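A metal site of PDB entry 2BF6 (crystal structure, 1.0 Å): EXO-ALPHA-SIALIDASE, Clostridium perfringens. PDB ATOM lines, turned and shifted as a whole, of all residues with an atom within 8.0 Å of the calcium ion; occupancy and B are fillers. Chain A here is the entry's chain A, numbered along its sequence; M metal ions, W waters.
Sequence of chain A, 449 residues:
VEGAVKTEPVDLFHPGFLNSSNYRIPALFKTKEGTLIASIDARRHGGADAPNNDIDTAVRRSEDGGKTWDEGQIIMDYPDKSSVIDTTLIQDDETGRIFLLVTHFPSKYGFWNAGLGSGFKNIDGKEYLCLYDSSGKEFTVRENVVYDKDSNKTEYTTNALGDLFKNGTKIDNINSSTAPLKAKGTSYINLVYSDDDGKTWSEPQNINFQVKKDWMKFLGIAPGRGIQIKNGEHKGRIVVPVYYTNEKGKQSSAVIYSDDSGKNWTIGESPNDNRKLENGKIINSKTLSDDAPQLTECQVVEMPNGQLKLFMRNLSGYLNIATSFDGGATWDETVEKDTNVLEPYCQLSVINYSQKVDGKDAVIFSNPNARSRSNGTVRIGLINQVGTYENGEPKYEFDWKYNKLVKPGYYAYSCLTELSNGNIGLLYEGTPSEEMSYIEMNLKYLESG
Within 4 Å of the calcium ion: Asp 54, Asp 56, Asp 77 and Tyr 78.
The calcium ion is bound by OD1 of Asp 54 (2.3 Å), OD1 of Asp 77 (2.3 Å), O of Tyr 78 (2.4 Å), OD1 of Asp 56 (2.4 Å), water W3 (2.4 Å), water W2 (2.5 Å) and water W1 (2.5 Å). The calcium ion has seven donor atoms within binding distance.
Water W2 lies within hydrogen-bond range of O of Ser 82 (2.7 Å), O of Ile 55 (2.8 Å) and N of Tyr 78 (2.9 Å).
The backbone carbonyl oxygen of Asp 54 sits at hydrogen-bond distance from the backbone NH of Arg 44 (3.0 Å). The side-chain carboxylate (OD2) of Asp 54 sits at hydrogen-bond distance from the backbone NH (N) of Lys 81, 2.9 Å away. OD2 of Asp 56 lies within salt-bridge range of NE of Arg 44 (2.8 Å). The backbone carbonyl oxygen (O) of Asp 56 is in hydrogen-bond range of the backbone NH (N) of Ala 42 (2.8 Å).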
ATOM      1  N   ALA A  42      34.446 -22.081 -21.944  1.00  0.00           N
ATOM      2  CA  ALA A  42      35.097 -23.053 -22.814  1.00  0.00           C
ATOM      3  C   ALA A  42      34.041 -23.497 -23.823  1.00  0.00           C
ATOM      4  O   ALA A  42      33.137 -24.300 -23.531  1.00  0.00           O
ATOM      5  CB  ALA A  42      35.615 -24.226 -22.038  1.00  0.00           C
ATOM      6  N   ARG A  44      32.924 -25.315 -26.897  1.00  0.00           N
ATOM      7  CA  ARG A  44      33.505 -26.519 -27.450  1.00  0.00           C
ATOM      8  C   ARG A  44      33.325 -26.696 -28.947  1.00  0.00           C
ATOM      9  O   ARG A  44      34.063 -27.465 -29.562  1.00  0.00           O
ATOM     10  CB  ARG A  44      32.945 -27.769 -26.776  1.00  0.00           C
ATOM     11  CG  ARG A  44      33.127 -27.833 -25.312  1.00  0.00           C
ATOM     12  CD  ARG A  44      34.528 -27.966 -24.884  1.00  0.00           C
ATOM     13  NE  ARG A  44      34.673 -28.294 -23.489  1.00  0.00           N
ATOM     14  CZ  ARG A  44      35.774 -28.700 -22.888  1.00  0.00           C
ATOM     15  NH1 ARG A  44      36.897 -28.904 -23.580  1.00  0.00           N
ATOM     16  NH2 ARG A  44      35.743 -28.894 -21.569  1.00  0.00           N
ATOM     17  N   HIS A  45      32.368 -26.024 -29.541  1.00  0.00           N
ATOM     18  CA  HIS A  45      32.021 -26.241 -30.938  1.00  0.00           C
ATOM     19  C   HIS A  45      32.055 -24.953 -31.691  1.00  0.00           C
ATOM     20  O   HIS A  45      31.269 -24.782 -32.588  1.00  0.00           O
ATOM     21  CB  HIS A  45      30.653 -26.909 -31.092  1.00  0.00           C
ATOM     22  CG  HIS A  45      30.576 -28.206 -30.380  1.00  0.00           C
ATOM     23  ND1 HIS A  45      29.641 -28.627 -29.496  1.00  0.00           N
ATOM     24  CD2 HIS A  45      31.461 -29.222 -30.555  1.00  0.00           C
ATOM     25  CE1 HIS A  45      29.887 -29.880 -29.077  1.00  0.00           C
ATOM     26  NE2 HIS A  45      31.012 -30.220 -29.696  1.00  0.00           N
ATOM     27  N   ASN A  53      25.872 -24.371 -29.493  1.00  0.00           N
ATOM     28  CA  ASN A  53      27.182 -24.761 -28.933  1.00  0.00           C
ATOM     29  C   ASN A  53      26.966 -25.732 -27.802  1.00  0.00           C
ATOM     30  O   ASN A  53      25.823 -26.097 -27.423  1.00  0.00           O
ATOM     31  CB  ASN A  53      27.926 -23.485 -28.491  1.00  0.00           C
ATOM     32  CG  ASN A  53      29.395 -23.584 -28.738  1.00  0.00           C
ATOM     33  OD1 ASN A  53      29.999 -24.640 -28.592  1.00  0.00           O
ATOM     34  ND2 ASN A  53      29.983 -22.446 -29.100  1.00  0.00           N
ATOM     35  N   ASP A  54      28.072 -26.101 -27.185  1.00  0.00           N
ATOM     36  CA  ASP A  54      28.125 -26.863 -25.917  1.00  0.00           C
ATOM     37  C   ASP A  54      29.235 -26.167 -25.137  1.00  0.00           C
ATOM     38  O   ASP A  54      30.395 -26.259 -25.516  1.00  0.00           O
ATOM     39  CB  ASP A  54      28.357 -28.339 -26.154  1.00  0.00           C
ATOM     40  CG  ASP A  54      28.159 -29.205 -24.934  1.00  0.00           C
ATOM     41  OD1 ASP A  54      28.505 -28.738 -23.824  1.00  0.00           O
ATOM     42  OD2 ASP A  54      27.702 -30.371 -25.120  1.00  0.00           O
ATOM     43  N   ILE A  55      28.858 -25.431 -24.110  1.00  0.00           N
ATOM     44  CA  ILE A  55      29.756 -24.522 -23.418  1.00  0.00           C
ATOM     45  C   ILE A  55      29.874 -24.950 -21.964  1.00  0.00           C
ATOM     46  O   ILE A  55      28.874 -25.182 -21.282  1.00  0.00           O
ATOM     47  CB  ILE A  55      29.283 -23.062 -23.524  1.00  0.00           C
ATOM     48  CG1 ILE A  55      29.009 -22.655 -24.938  1.00  0.00           C
ATOM     49  CG2 ILE A  55      30.300 -22.140 -22.846  1.00  0.00           C
ATOM     50  CD1 ILE A  55      28.339 -21.339 -25.154  1.00  0.00           C
ATOM     51  N   ASP A  56      31.129 -25.047 -21.493  1.00  0.00           N
ATOM     52  CA  ASP A  56      31.496 -25.373 -20.126  1.00  0.00           C
ATOM     53  C   ASP A  56      32.163 -24.181 -19.464  1.00  0.00           C
ATOM     54  O   ASP A  56      32.657 -23.295 -20.170  1.00  0.00           O
ATOM     55  CB  ASP A  56      32.467 -26.562 -20.149  1.00  0.00           C
ATOM     56  CG  ASP A  56      31.970 -27.776 -20.896  1.00  0.00           C
ATOM     57  OD1 ASP A  56      30.724 -27.994 -20.900  1.00  0.00           O
ATOM     58  OD2 ASP A  56      32.805 -28.525 -21.408  1.00  0.00           O
ATOM     59  N   THR A  57      32.232 -24.147 -18.146  1.00  0.00           N
ATOM     60  CA  THR A  57      32.920 -23.092 -17.428  1.00  0.00           C
ATOM     61  C   THR A  57      34.306 -23.569 -17.010  1.00  0.00           C
ATOM     62  O   THR A  57      34.441 -24.626 -16.381  1.00  0.00           O
ATOM     63  CB  THR A  57      32.144 -22.670 -16.152  1.00  0.00           C
ATOM     64  OG1 THR A  57      30.885 -22.221 -16.472  1.00  0.00           O
ATOM     65  CG2 THR A  57      32.953 -21.595 -15.413  1.00  0.00           C
ATOM     66  N   ILE A  74      37.758 -27.483 -15.453  1.00  0.00           N
ATOM     67  CA  ILE A  74      36.354 -27.309 -15.806  1.00  0.00           C
ATOM     68  C   ILE A  74      35.531 -27.507 -14.561  1.00  0.00           C
ATOM     69  O   ILE A  74      35.694 -28.522 -13.873  1.00  0.00           O
ATOM     70  CB  ILE A  74      35.964 -28.326 -16.882  1.00  0.00           C
ATOM     71  CG1 ILE A  74      36.810 -28.196 -18.140  1.00  0.00           C
ATOM     72  CG2 ILE A  74      34.450 -28.186 -17.176  1.00  0.00           C
ATOM     73  CD1 ILE A  74      36.629 -26.890 -18.858  1.00  0.00           C
ATOM     74  N   MET A  76      31.924 -26.598 -14.425  1.00  0.00           N
ATOM     75  CA  MET A  76      30.560 -26.935 -14.752  1.00  0.00           C
ATOM     76  C   MET A  76      30.553 -27.406 -16.213  1.00  0.00           C
ATOM     77  O   MET A  76      31.101 -26.722 -17.088  1.00  0.00           O
ATOM     78  CB  MET A  76      29.560 -25.759 -14.617  1.00  0.00           C
ATOM     79  CG  MET A  76      29.066 -25.563 -13.183  1.00  0.00           C
ATOM     80  SD  MET A  76      28.122 -24.037 -12.920  1.00  0.00           S
ATOM     81  CE  MET A  76      29.423 -22.848 -12.961  1.00  0.00           C
ATOM     82  N   ASP A  77      29.924 -28.556 -16.462  1.00  0.00           N
ATOM     83  CA  ASP A  77      29.856 -29.183 -17.783  1.00  0.00           C
ATOM     84  C   ASP A  77      28.576 -29.991 -17.828  1.00  0.00           C
ATOM     85  O   ASP A  77      28.472 -31.016 -17.176  1.00  0.00           O
ATOM     86  CB  ASP A  77      31.070 -30.077 -18.016  1.00  0.00           C
ATOM     87  CG  ASP A  77      31.078 -30.911 -19.278  1.00  0.00           C
ATOM     88  OD1 ASP A  77      30.074 -30.866 -20.028  1.00  0.00           O
ATOM     89  OD2 ASP A  77      32.061 -31.680 -19.424  1.00  0.00           O
ATOM     90  N   TYR A  78      27.592 -29.528 -18.602  1.00  0.00           N
ATOM     91  CA  TYR A  78      26.366 -30.224 -18.839  1.00  0.00           C
ATOM     92  C   TYR A  78      26.430 -30.957 -20.176  1.00  0.00           C
ATOM     93  O   TYR A  78      27.165 -30.575 -21.088  1.00  0.00           O
ATOM     94  CB  TYR A  78      25.215 -29.225 -18.826  1.00  0.00           C
ATOM     95  CG  TYR A  78      24.973 -28.626 -17.474  1.00  0.00           C
ATOM     96  CD1 TYR A  78      25.604 -27.464 -17.064  1.00  0.00           C
ATOM     97  CD2 TYR A  78      24.119 -29.241 -16.558  1.00  0.00           C
ATOM     98  CE1 TYR A  78      25.389 -26.943 -15.819  1.00  0.00           C
ATOM     99  CE2 TYR A  78      23.868 -28.705 -15.334  1.00  0.00           C
ATOM    100  CZ  TYR A  78      24.507 -27.542 -14.947  1.00  0.00           C
ATOM    101  OH  TYR A  78      24.285 -26.950 -13.736  1.00  0.00           O
ATOM    102  N   PRO A  79      25.638 -32.019 -20.334  1.00  0.00           N
ATOM    103  CA  PRO A  79      25.739 -32.789 -21.561  1.00  0.00           C
ATOM    104  C   PRO A  79      24.909 -32.239 -22.723  1.00  0.00           C
ATOM    105  O   PRO A  79      23.987 -31.443 -22.520  1.00  0.00           O
ATOM    106  CB  PRO A  79      25.131 -34.152 -21.109  1.00  0.00           C
ATOM    107  CG  PRO A  79      24.090 -33.754 -20.099  1.00  0.00           C
ATOM    108  CD  PRO A  79      24.722 -32.594 -19.334  1.00  0.00           C
ATOM    109  N   ASP A  80      25.240 -32.750 -23.906  1.00  0.00           N
ATOM    110  CA  ASP A  80      24.305 -32.711 -25.038  1.00  0.00           C
ATOM    111  C   ASP A  80      23.845 -31.311 -25.364  1.00  0.00           C
ATOM    112  O   ASP A  80      22.663 -31.074 -25.616  1.00  0.00           O
ATOM    113  CB  ASP A  80      23.111 -33.621 -24.799  1.00  0.00           C
ATOM    114  CG  ASP A  80      22.279 -33.888 -26.011  1.00  0.00           C
ATOM    115  OD1 ASP A  80      22.774 -33.797 -27.159  1.00  0.00           O
ATOM    116  OD2 ASP A  80      21.075 -34.245 -25.830  1.00  0.00           O
ATOM    117  N   LYS A  81      24.789 -30.351 -25.435  1.00  0.00           N
ATOM    118  CA  LYS A  81      24.511 -29.000 -25.882  1.00  0.00           C
ATOM    119  C   LYS A  81      23.667 -28.200 -24.900  1.00  0.00           C
ATOM    120  O   LYS A  81      23.137 -27.142 -25.258  1.00  0.00           O
ATOM    121  CB  LYS A  81      23.998 -28.899 -27.316  1.00  0.00           C
ATOM    122  CG  LYS A  81      24.906 -29.528 -28.353  1.00  0.00           C
ATOM    123  CD  LYS A  81      24.348 -29.439 -29.751  1.00  0.00           C
ATOM    124  CE  LYS A  81      24.208 -27.994 -30.280  1.00  0.00           C
ATOM    125  NZ  LYS A  81      23.510 -27.976 -31.552  1.00  0.00           N
ATOM    126  N   SER A  82      23.585 -28.637 -23.649  1.00  0.00           N
ATOM    127  CA  SER A  82      23.207 -27.759 -22.546  1.00  0.00           C
ATOM    128  C   SER A  82      24.434 -26.951 -22.170  1.00  0.00           C
ATOM    129  O   SER A  82      25.494 -27.560 -22.021  1.00  0.00           O
ATOM    130  CB  SER A  82      22.710 -28.583 -21.389  1.00  0.00           C
ATOM    131  OG  SER A  82      22.438 -27.766 -20.266  1.00  0.00           O
ATOM    132  N   SER A  83      24.307 -25.643 -22.039  1.00  0.00           N
ATOM    133  CA  SER A  83      25.440 -24.752 -21.864  1.00  0.00           C
ATOM    134  C   SER A  83      25.341 -23.922 -20.598  1.00  0.00           C
ATOM    135  O   SER A  83      24.259 -23.487 -20.209  1.00  0.00           O
ATOM    136  CB  SER A  83      25.569 -23.781 -23.045  1.00  0.00           C
ATOM    137  OG  SER A  83      26.047 -24.454 -24.194  1.00  0.00           O
ATOM    138  N   VAL A  84      26.509 -23.633 -20.047  1.00  0.00           N
ATOM    139  CA  VAL A  84      26.694 -22.553 -19.073  1.00  0.00           C
ATOM    140  C   VAL A  84      27.465 -21.453 -19.763  1.00  0.00           C
ATOM    141  O   VAL A  84      28.501 -21.715 -20.410  1.00  0.00           O
ATOM    142  CB  VAL A  84      27.398 -23.025 -17.787  1.00  0.00           C
ATOM    143  CG1 VAL A  84      26.403 -23.639 -16.846  1.00  0.00           C
ATOM    144  CG2 VAL A  84      28.558 -23.981 -18.071  1.00  0.00           C
HETATM  145 CA    CA M   1      29.219 -29.620 -21.803  1.00  0.00          CA
HETATM  146  O   HOH W   1      28.950 -31.707 -23.133  1.00  0.00           O
HETATM  147  O   HOH W   2      27.950 -27.741 -20.865  1.00  0.00           O
HETATM  148  O   HOH W   3      31.323 -30.124 -22.915  1.00  0.00           O
